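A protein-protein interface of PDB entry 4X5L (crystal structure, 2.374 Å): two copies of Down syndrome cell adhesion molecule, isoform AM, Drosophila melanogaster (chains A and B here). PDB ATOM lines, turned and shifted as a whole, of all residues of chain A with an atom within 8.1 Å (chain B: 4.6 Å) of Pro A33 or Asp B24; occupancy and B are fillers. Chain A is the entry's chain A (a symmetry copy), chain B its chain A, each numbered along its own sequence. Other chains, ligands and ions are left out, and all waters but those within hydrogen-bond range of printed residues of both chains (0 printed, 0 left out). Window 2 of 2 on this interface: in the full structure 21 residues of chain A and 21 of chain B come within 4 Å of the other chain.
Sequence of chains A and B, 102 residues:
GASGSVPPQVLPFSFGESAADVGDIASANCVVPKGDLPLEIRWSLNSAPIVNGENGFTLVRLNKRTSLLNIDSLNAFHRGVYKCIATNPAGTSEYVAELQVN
Of the printed residues of chain A, Asp B24 touches Pro A33 (3.98 Å) and Lys A34 (3.1 Å).
No residue of chain A comes within 4 Å of Gly B23.
Of chain A, only Val A31, Pro A33, Arg A65 and Thr A66 come within 4 Å of Ile B25.
Printed residues of chain B within 4 Å of Lys A34: Asp B21 and Asp B24.
Printed residues of chain B within 4 Å of Arg A65: Ile B25 (3.7 Å).
The nearest printed residue of chain A that does not touch Asp B72 is Thr A66 (6.5 Å).
The guanidinium group (NH2) of Arg A65 sits at hydrogen-bond distance from the backbone carbonyl oxygen (O) of Gly A35, at 3.0 Å.
The backbone NH of Val A32 lies within hydrogen-bond range of the backbone carbonyl oxygen of Arg A65 (2.7 Å).
The backbone NH (N) of Gln A9 is in hydrogen-bond range of the backbone carbonyl oxygen (O) of Lys A34 (3.2 Å).
The side-chain amide oxygen (OD1) of Asn A63 sits at hydrogen-bond distance from the backbone NH (N) of Arg A65 (2.6 Å).
N of Leu A11 lies within hydrogen-bond range of O of Val A31 (3.1 Å).
O of Asp B24 is in hydrogen-bond range of N of Leu B74, at 2.9 Å.
Among the printed residues, pairs that only touch across the chains: Val A31 with Ile B25, Pro A33 with Asp B24, Pro A33 with Ile B25, Arg A65 with Ile B25 and Thr A66 with Ile B25.
Of the 19 printed residues of chain A, 6 touch a printed residue of chain B.
Hydrophobic or aromatic side chains of chain A within 4 Å of the printed part of chain B: Val A31 and Pro A33.
Hydrophobic or aromatic side chains of chain B that line the printed part of chain A: Ile B25.
Among the printed residues, 8 pairs touch across the chains.
Among the printed residues, Asp or Glu carboxylates within 4 Å of a Lys or Arg side-chain nitrogen of the other chain: Lys A34 with Asp B21 (3.7 Å) and Lys A34 with Asp B24 (3.1 Å).
The side-chain carboxylate (OD1) of Asp B72 is in hydrogen-bond range of the side-chain amide nitrogen (ND2) of Asn A63, at 2.7 Å.
OD2 of Asp B21 lies within salt-bridge range of NZ of Lys A34 (3.7 Å).
The side-chain carboxylate (OD2) of Asp B24 lies within salt-bridge range of the side-chain amino group (NZ) of Lys A34, 3.1 Å away.
No position is printed for both chains.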
ATOM      1  N   PRO A   7     -10.821 -15.517  13.592  1.00  0.00           N
ATOM      2  CA  PRO A   7      -9.387 -15.249  13.753  1.00  0.00           C
ATOM      3  C   PRO A   7      -8.539 -16.351  13.124  1.00  0.00           C
ATOM      4  O   PRO A   7      -9.073 -17.409  12.794  1.00  0.00           O
ATOM      5  CB  PRO A   7      -9.206 -15.205  15.273  1.00  0.00           C
ATOM      6  CG  PRO A   7     -10.287 -16.073  15.800  1.00  0.00           C
ATOM      7  CD  PRO A   7     -11.454 -15.899  14.868  1.00  0.00           C
ATOM      8  N   PRO A   8      -7.230 -16.110  12.960  1.00  0.00           N
ATOM      9  CA  PRO A   8      -6.365 -17.089  12.298  1.00  0.00           C
ATOM     10  C   PRO A   8      -5.955 -18.237  13.214  1.00  0.00           C
ATOM     11  O   PRO A   8      -6.109 -18.141  14.431  1.00  0.00           O
ATOM     12  CB  PRO A   8      -5.150 -16.256  11.895  1.00  0.00           C
ATOM     13  CG  PRO A   8      -5.062 -15.210  12.952  1.00  0.00           C
ATOM     14  CD  PRO A   8      -6.481 -14.907  13.369  1.00  0.00           C
ATOM     15  N   GLN A   9      -5.452 -19.314  12.619  1.00  0.00           N
ATOM     16  CA  GLN A   9      -4.880 -20.420  13.376  1.00  0.00           C
ATOM     17  C   GLN A   9      -3.670 -20.969  12.632  1.00  0.00           C
ATOM     18  O   GLN A   9      -3.803 -21.565  11.563  1.00  0.00           O
ATOM     19  CB  GLN A   9      -5.912 -21.527  13.607  1.00  0.00           C
ATOM     20  CG  GLN A   9      -5.395 -22.688  14.450  1.00  0.00           C
ATOM     21  CD  GLN A   9      -5.043 -22.273  15.867  1.00  0.00           C
ATOM     22  OE1 GLN A   9      -3.882 -22.323  16.272  1.00  0.00           O
ATOM     23  NE2 GLN A   9      -6.051 -21.865  16.631  1.00  0.00           N
ATOM     24  N   VAL A  10      -2.491 -20.754  13.202  1.00  0.00           N
ATOM     25  CA  VAL A  10      -1.249 -21.223  12.602  1.00  0.00           C
ATOM     26  C   VAL A  10      -1.013 -22.687  12.961  1.00  0.00           C
ATOM     27  O   VAL A  10      -0.889 -23.034  14.136  1.00  0.00           O
ATOM     28  CB  VAL A  10      -0.046 -20.370  13.064  1.00  0.00           C
ATOM     29  CG1 VAL A  10       1.262 -20.908  12.490  1.00  0.00           C
ATOM     30  CG2 VAL A  10      -0.243 -18.918  12.661  1.00  0.00           C
ATOM     31  N   LEU A  11      -0.962 -23.541  11.944  1.00  0.00           N
ATOM     32  CA  LEU A  11      -0.674 -24.954  12.150  1.00  0.00           C
ATOM     33  C   LEU A  11       0.729 -25.127  12.718  1.00  0.00           C
ATOM     34  O   LEU A  11       1.593 -24.278  12.498  1.00  0.00           O
ATOM     35  CB  LEU A  11      -0.801 -25.733  10.840  1.00  0.00           C
ATOM     36  CG  LEU A  11      -2.169 -25.765  10.160  1.00  0.00           C
ATOM     37  CD1 LEU A  11      -2.059 -26.488   8.827  1.00  0.00           C
ATOM     38  CD2 LEU A  11      -3.209 -26.434  11.046  1.00  0.00           C
ATOM     39  N   PRO A  12       0.964 -26.227  13.454  1.00  0.00           N
ATOM     40  CA  PRO A  12       2.323 -26.491  13.937  1.00  0.00           C
ATOM     41  C   PRO A  12       3.311 -26.613  12.783  1.00  0.00           C
ATOM     42  O   PRO A  12       2.929 -27.066  11.704  1.00  0.00           O
ATOM     43  CB  PRO A  12       2.184 -27.825  14.681  1.00  0.00           C
ATOM     44  CG  PRO A  12       0.736 -27.955  14.995  1.00  0.00           C
ATOM     45  CD  PRO A  12       0.012 -27.261  13.890  1.00  0.00           C
ATOM     46  N   CYS A  30       5.136 -21.931   7.413  1.00  0.00           N
ATOM     47  CA  CYS A  30       3.997 -21.446   8.182  1.00  0.00           C
ATOM     48  C   CYS A  30       2.729 -21.497   7.336  1.00  0.00           C
ATOM     49  O   CYS A  30       2.662 -20.879   6.273  1.00  0.00           O
ATOM     50  CB  CYS A  30       4.245 -20.020   8.675  1.00  0.00           C
ATOM     51  SG  CYS A  30       2.868 -19.311   9.606  1.00  0.00           S
ATOM     52  N   VAL A  31       1.729 -22.233   7.814  1.00  0.00           N
ATOM     53  CA  VAL A  31       0.480 -22.418   7.080  1.00  0.00           C
ATOM     54  C   VAL A  31      -0.705 -21.932   7.911  1.00  0.00           C
ATOM     55  O   VAL A  31      -0.821 -22.258   9.092  1.00  0.00           O
ATOM     56  CB  VAL A  31       0.267 -23.897   6.698  1.00  0.00           C
ATOM     57  CG1 VAL A  31      -0.923 -24.042   5.760  1.00  0.00           C
ATOM     58  CG2 VAL A  31       1.523 -24.461   6.049  1.00  0.00           C
ATOM     59  N   VAL A  32      -1.581 -21.155   7.280  1.00  0.00           N
ATOM     60  CA  VAL A  32      -2.742 -20.580   7.955  1.00  0.00           C
ATOM     61  C   VAL A  32      -4.013 -20.906   7.168  1.00  0.00           C
ATOM     62  O   VAL A  32      -4.597 -20.029   6.533  1.00  0.00           O
ATOM     63  CB  VAL A  32      -2.601 -19.049   8.116  1.00  0.00           C
ATOM     64  CG1 VAL A  32      -3.664 -18.514   9.064  1.00  0.00           C
ATOM     65  CG2 VAL A  32      -1.208 -18.690   8.625  1.00  0.00           C
ATOM     66  N   PRO A  33      -4.450 -22.175   7.217  1.00  0.00           N
ATOM     67  CA  PRO A  33      -5.556 -22.642   6.373  1.00  0.00           C
ATOM     68  C   PRO A  33      -6.913 -22.072   6.772  1.00  0.00           C
ATOM     69  O   PRO A  33      -7.849 -22.113   5.972  1.00  0.00           O
ATOM     70  CB  PRO A  33      -5.528 -24.155   6.581  1.00  0.00           C
ATOM     71  CG  PRO A  33      -5.013 -24.319   7.963  1.00  0.00           C
ATOM     72  CD  PRO A  33      -3.999 -23.222   8.152  1.00  0.00           C
ATOM     73  N   LYS A  34      -7.014 -21.551   7.992  1.00  0.00           N
ATOM     74  CA  LYS A  34      -8.268 -21.001   8.493  1.00  0.00           C
ATOM     75  C   LYS A  34      -8.056 -19.661   9.185  1.00  0.00           C
ATOM     76  O   LYS A  34      -7.084 -19.471   9.917  1.00  0.00           O
ATOM     77  CB  LYS A  34      -8.937 -21.991   9.447  1.00  0.00           C
ATOM     78  CG  LYS A  34      -9.620 -23.142   8.731  1.00  0.00           C
ATOM     79  CD  LYS A  34     -10.451 -23.986   9.682  1.00  0.00           C
ATOM     80  CE  LYS A  34     -11.268 -25.027   8.932  1.00  0.00           C
ATOM     81  NZ  LYS A  34     -12.215 -24.411   7.957  1.00  0.00           N
ATOM     82  N   GLY A  35      -8.985 -18.741   8.943  1.00  0.00           N
ATOM     83  CA  GLY A  35      -8.889 -17.384   9.448  1.00  0.00           C
ATOM     84  C   GLY A  35      -9.297 -16.398   8.374  1.00  0.00           C
ATOM     85  O   GLY A  35      -8.975 -16.584   7.200  1.00  0.00           O
ATOM     86  N   ASP A  36     -10.013 -15.351   8.771  1.00  0.00           N
ATOM     87  CA  ASP A  36     -10.476 -14.342   7.827  1.00  0.00           C
ATOM     88  C   ASP A  36      -9.315 -13.658   7.114  1.00  0.00           C
ATOM     89  O   ASP A  36      -8.256 -13.436   7.699  1.00  0.00           O
ATOM     90  CB  ASP A  36     -11.328 -13.287   8.538  1.00  0.00           C
ATOM     91  CG  ASP A  36     -12.768 -13.728   8.736  1.00  0.00           C
ATOM     92  OD1 ASP A  36     -13.289 -14.497   7.900  1.00  0.00           O
ATOM     93  OD2 ASP A  36     -13.385 -13.290   9.729  1.00  0.00           O
ATOM     94  N   LEU A  39      -4.619 -11.567   5.579  1.00  0.00           N
ATOM     95  CA  LEU A  39      -3.756 -12.062   6.649  1.00  0.00           C
ATOM     96  C   LEU A  39      -2.361 -11.446   6.605  1.00  0.00           C
ATOM     97  O   LEU A  39      -1.729 -11.385   5.549  1.00  0.00           O
ATOM     98  CB  LEU A  39      -3.636 -13.586   6.574  1.00  0.00           C
ATOM     99  CG  LEU A  39      -4.844 -14.400   7.041  1.00  0.00           C
ATOM    100  CD1 LEU A  39      -4.662 -15.864   6.677  1.00  0.00           C
ATOM    101  CD2 LEU A  39      -5.056 -14.247   8.536  1.00  0.00           C
ATOM    102  N   ILE A  41       1.370 -12.066   7.824  1.00  0.00           N
ATOM    103  CA  ILE A  41       2.223 -13.164   8.269  1.00  0.00           C
ATOM    104  C   ILE A  41       3.679 -12.706   8.325  1.00  0.00           C
ATOM    105  O   ILE A  41       4.263 -12.336   7.305  1.00  0.00           O
ATOM    106  CB  ILE A  41       2.088 -14.391   7.345  1.00  0.00           C
ATOM    107  CG1 ILE A  41       0.626 -14.846   7.287  1.00  0.00           C
ATOM    108  CG2 ILE A  41       2.974 -15.531   7.837  1.00  0.00           C
ATOM    109  CD1 ILE A  41       0.343 -15.941   6.275  1.00  0.00           C
ATOM    110  N   ASN A  63       1.700 -18.078  -0.964  1.00  0.00           N
ATOM    111  CA  ASN A  63       0.245 -18.061  -0.942  1.00  0.00           C
ATOM    112  C   ASN A  63      -0.252 -17.017   0.051  1.00  0.00           C
ATOM    113  O   ASN A  63       0.516 -16.529   0.879  1.00  0.00           O
ATOM    114  CB  ASN A  63      -0.297 -19.444  -0.576  1.00  0.00           C
ATOM    115  CG  ASN A  63      -1.802 -19.544  -0.722  1.00  0.00           C
ATOM    116  OD1 ASN A  63      -2.552 -19.079   0.137  1.00  0.00           O
ATOM    117  ND2 ASN A  63      -2.253 -20.161  -1.808  1.00  0.00           N
ATOM    118  N   LYS A  64      -1.532 -16.670  -0.032  1.00  0.00           N
ATOM    119  CA  LYS A  64      -2.133 -15.750   0.928  1.00  0.00           C
ATOM    120  C   LYS A  64      -2.257 -16.394   2.307  1.00  0.00           C
ATOM    121  O   LYS A  64      -2.456 -15.700   3.306  1.00  0.00           O
ATOM    122  CB  LYS A  64      -3.507 -15.289   0.440  1.00  0.00           C
ATOM    123  CG  LYS A  64      -3.487 -13.940  -0.256  1.00  0.00           C
ATOM    124  CD  LYS A  64      -4.770 -13.697  -1.032  1.00  0.00           C
ATOM    125  CE  LYS A  64      -4.642 -12.499  -1.957  1.00  0.00           C
ATOM    126  NZ  LYS A  64      -5.541 -12.613  -3.138  1.00  0.00           N
ATOM    127  N   ARG A  65      -2.135 -17.718   2.349  1.00  0.00           N
ATOM    128  CA  ARG A  65      -2.258 -18.478   3.588  1.00  0.00           C
ATOM    129  C   ARG A  65      -0.979 -19.242   3.917  1.00  0.00           C
ATOM    130  O   ARG A  65      -0.956 -20.055   4.844  1.00  0.00           O
ATOM    131  CB  ARG A  65      -3.430 -19.456   3.497  1.00  0.00           C
ATOM    132  CG  ARG A  65      -4.783 -18.785   3.374  1.00  0.00           C
ATOM    133  CD  ARG A  65      -5.908 -19.798   3.478  1.00  0.00           C
ATOM    134  NE  ARG A  65      -7.219 -19.158   3.528  1.00  0.00           N
ATOM    135  CZ  ARG A  65      -7.721 -18.558   4.603  1.00  0.00           C
ATOM    136  NH1 ARG A  65      -7.022 -18.500   5.730  1.00  0.00           N
ATOM    137  NH2 ARG A  65      -8.926 -18.008   4.550  1.00  0.00           N
ATOM    138  N   THR A  66       0.082 -18.985   3.155  1.00  0.00           N
ATOM    139  CA  THR A  66       1.354 -19.667   3.366  1.00  0.00           C
ATOM    140  C   THR A  66       2.536 -18.707   3.324  1.00  0.00           C
ATOM    141  O   THR A  66       2.581 -17.789   2.506  1.00  0.00           O
ATOM    142  CB  THR A  66       1.593 -20.762   2.311  1.00  0.00           C
ATOM    143  OG1 THR A  66       0.466 -21.645   2.270  1.00  0.00           O
ATOM    144  CG2 THR A  66       2.852 -21.562   2.642  1.00  0.00           C
ATOM    145  N   ASP B  21     -10.468 -29.628   5.954  1.00  0.00           N
ATOM    146  CA  ASP B  21     -11.766 -29.505   5.300  1.00  0.00           C
ATOM    147  C   ASP B  21     -11.627 -29.225   3.808  1.00  0.00           C
ATOM    148  O   ASP B  21     -10.600 -28.727   3.347  1.00  0.00           O
ATOM    149  CB  ASP B  21     -12.592 -28.397   5.959  1.00  0.00           C
ATOM    150  CG  ASP B  21     -13.189 -28.821   7.288  1.00  0.00           C
ATOM    151  OD1 ASP B  21     -13.652 -29.975   7.399  1.00  0.00           O
ATOM    152  OD2 ASP B  21     -13.196 -27.994   8.224  1.00  0.00           O
ATOM    153  N   VAL B  22     -12.674 -29.558   3.060  1.00  0.00           N
ATOM    154  CA  VAL B  22     -12.724 -29.278   1.631  1.00  0.00           C
ATOM    155  C   VAL B  22     -12.716 -27.773   1.402  1.00  0.00           C
ATOM    156  O   VAL B  22     -13.372 -27.022   2.124  1.00  0.00           O
ATOM    157  CB  VAL B  22     -13.979 -29.906   0.981  1.00  0.00           C
ATOM    158  CG1 VAL B  22     -14.199 -29.386  -0.442  1.00  0.00           C
ATOM    159  CG2 VAL B  22     -13.868 -31.420   0.980  1.00  0.00           C
ATOM    160  N   GLY B  23     -11.964 -27.341   0.396  1.00  0.00           N
ATOM    161  CA  GLY B  23     -11.875 -25.933   0.058  1.00  0.00           C
ATOM    162  C   GLY B  23     -10.740 -25.226   0.774  1.00  0.00           C
ATOM    163  O   GLY B  23     -10.377 -24.107   0.412  1.00  0.00           O
ATOM    164  N   ASP B  24     -10.178 -25.874   1.791  1.00  0.00           N
ATOM    165  CA  ASP B  24      -9.050 -25.308   2.523  1.00  0.00           C
ATOM    166  C   ASP B  24      -7.734 -25.620   1.826  1.00  0.00           C
ATOM    167  O   ASP B  24      -7.679 -26.460   0.925  1.00  0.00           O
ATOM    168  CB  ASP B  24      -9.012 -25.835   3.961  1.00  0.00           C
ATOM    169  CG  ASP B  24     -10.132 -25.277   4.817  1.00  0.00           C
ATOM    170  OD1 ASP B  24     -10.783 -24.300   4.395  1.00  0.00           O
ATOM    171  OD2 ASP B  24     -10.352 -25.813   5.922  1.00  0.00           O
ATOM    172  N   ILE B  25      -6.677 -24.938   2.256  1.00  0.00           N
ATOM    173  CA  ILE B  25      -5.353 -25.113   1.677  1.00  0.00           C
ATOM    174  C   ILE B  25      -4.509 -26.078   2.502  1.00  0.00           C
ATOM    175  O   ILE B  25      -4.646 -26.149   3.724  1.00  0.00           O
ATOM    176  CB  ILE B  25      -4.605 -23.768   1.565  1.00  0.00           C
ATOM    177  CG1 ILE B  25      -4.384 -23.151   2.949  1.00  0.00           C
ATOM    178  CG2 ILE B  25      -5.379 -22.800   0.689  1.00  0.00           C
ATOM    179  CD1 ILE B  25      -2.936 -23.105   3.372  1.00  0.00           C
ATOM    180  N   ALA B  26      -3.641 -26.824   1.824  1.00  0.00           N
ATOM    181  CA  ALA B  26      -2.684 -27.698   2.492  1.00  0.00           C
ATOM    182  C   ALA B  26      -1.289 -27.426   1.954  1.00  0.00           C
ATOM    183  O   ALA B  26      -1.121 -27.102   0.778  1.00  0.00           O
ATOM    184  CB  ALA B  26      -3.054 -29.156   2.299  1.00  0.00           C
ATOM    185  N   ILE B  71      -1.447 -27.070  -1.951  1.00  0.00           N
ATOM    186  CA  ILE B  71      -2.788 -27.320  -2.472  1.00  0.00           C
ATOM    187  C   ILE B  71      -3.669 -26.135  -2.091  1.00  0.00           C
ATOM    188  O   ILE B  71      -3.766 -25.783  -0.916  1.00  0.00           O
ATOM    189  CB  ILE B  71      -3.395 -28.634  -1.926  1.00  0.00           C
ATOM    190  CG1 ILE B  71      -2.413 -29.796  -2.118  1.00  0.00           C
ATOM    191  CG2 ILE B  71      -4.728 -28.932  -2.614  1.00  0.00           C
ATOM    192  CD1 ILE B  71      -2.833 -31.084  -1.440  1.00  0.00           C
ATOM    193  N   ASP B  72      -4.312 -25.527  -3.084  1.00  0.00           N
ATOM    194  CA  ASP B  72      -5.042 -24.276  -2.878  1.00  0.00           C
ATOM    195  C   ASP B  72      -6.525 -24.507  -2.599  1.00  0.00           C
ATOM    196  O   ASP B  72      -7.200 -23.644  -2.042  1.00  0.00           O
ATOM    197  CB  ASP B  72      -4.900 -23.359  -4.098  1.00  0.00           C
ATOM    198  CG  ASP B  72      -3.517 -22.741  -4.215  1.00  0.00           C
ATOM    199  OD1 ASP B  72      -2.952 -22.321  -3.183  1.00  0.00           O
ATOM    200  OD2 ASP B  72      -2.998 -22.668  -5.348  1.00  0.00           O
ATOM    201  N   SER B  73      -7.030 -25.666  -3.009  1.00  0.00           N
ATOM    202  CA  SER B  73      -8.429 -26.010  -2.780  1.00  0.00           C
ATOM    203  C   SER B  73      -8.596 -27.520  -2.655  1.00  0.00           C
ATOM    204  O   SER B  73      -8.807 -28.220  -3.646  1.00  0.00           O
ATOM    205  CB  SER B  73      -9.305 -25.466  -3.910  1.00  0.00           C
ATOM    206  OG  SER B  73     -10.679 -25.680  -3.645  1.00  0.00           O
ATOM    207  N   LEU B  74      -8.496 -28.012  -1.424  1.00  0.00           N
ATOM    208  CA  LEU B  74      -8.574 -29.442  -1.148  1.00  0.00           C
ATOM    209  C   LEU B  74      -9.911 -30.047  -1.560  1.00  0.00           C
ATOM    210  O   LEU B  74     -10.955 -29.406  -1.458  1.00  0.00           O
ATOM    211  CB  LEU B  74      -8.342 -29.707   0.342  1.00  0.00           C
ATOM    212  CG  LEU B  74      -6.911 -29.584   0.863  1.00  0.00           C
ATOM    213  CD1 LEU B  74      -6.930 -29.460   2.376  1.00  0.00           C
ATOM    214  CD2 LEU B  74      -6.073 -30.782   0.435  1.00  0.00           C
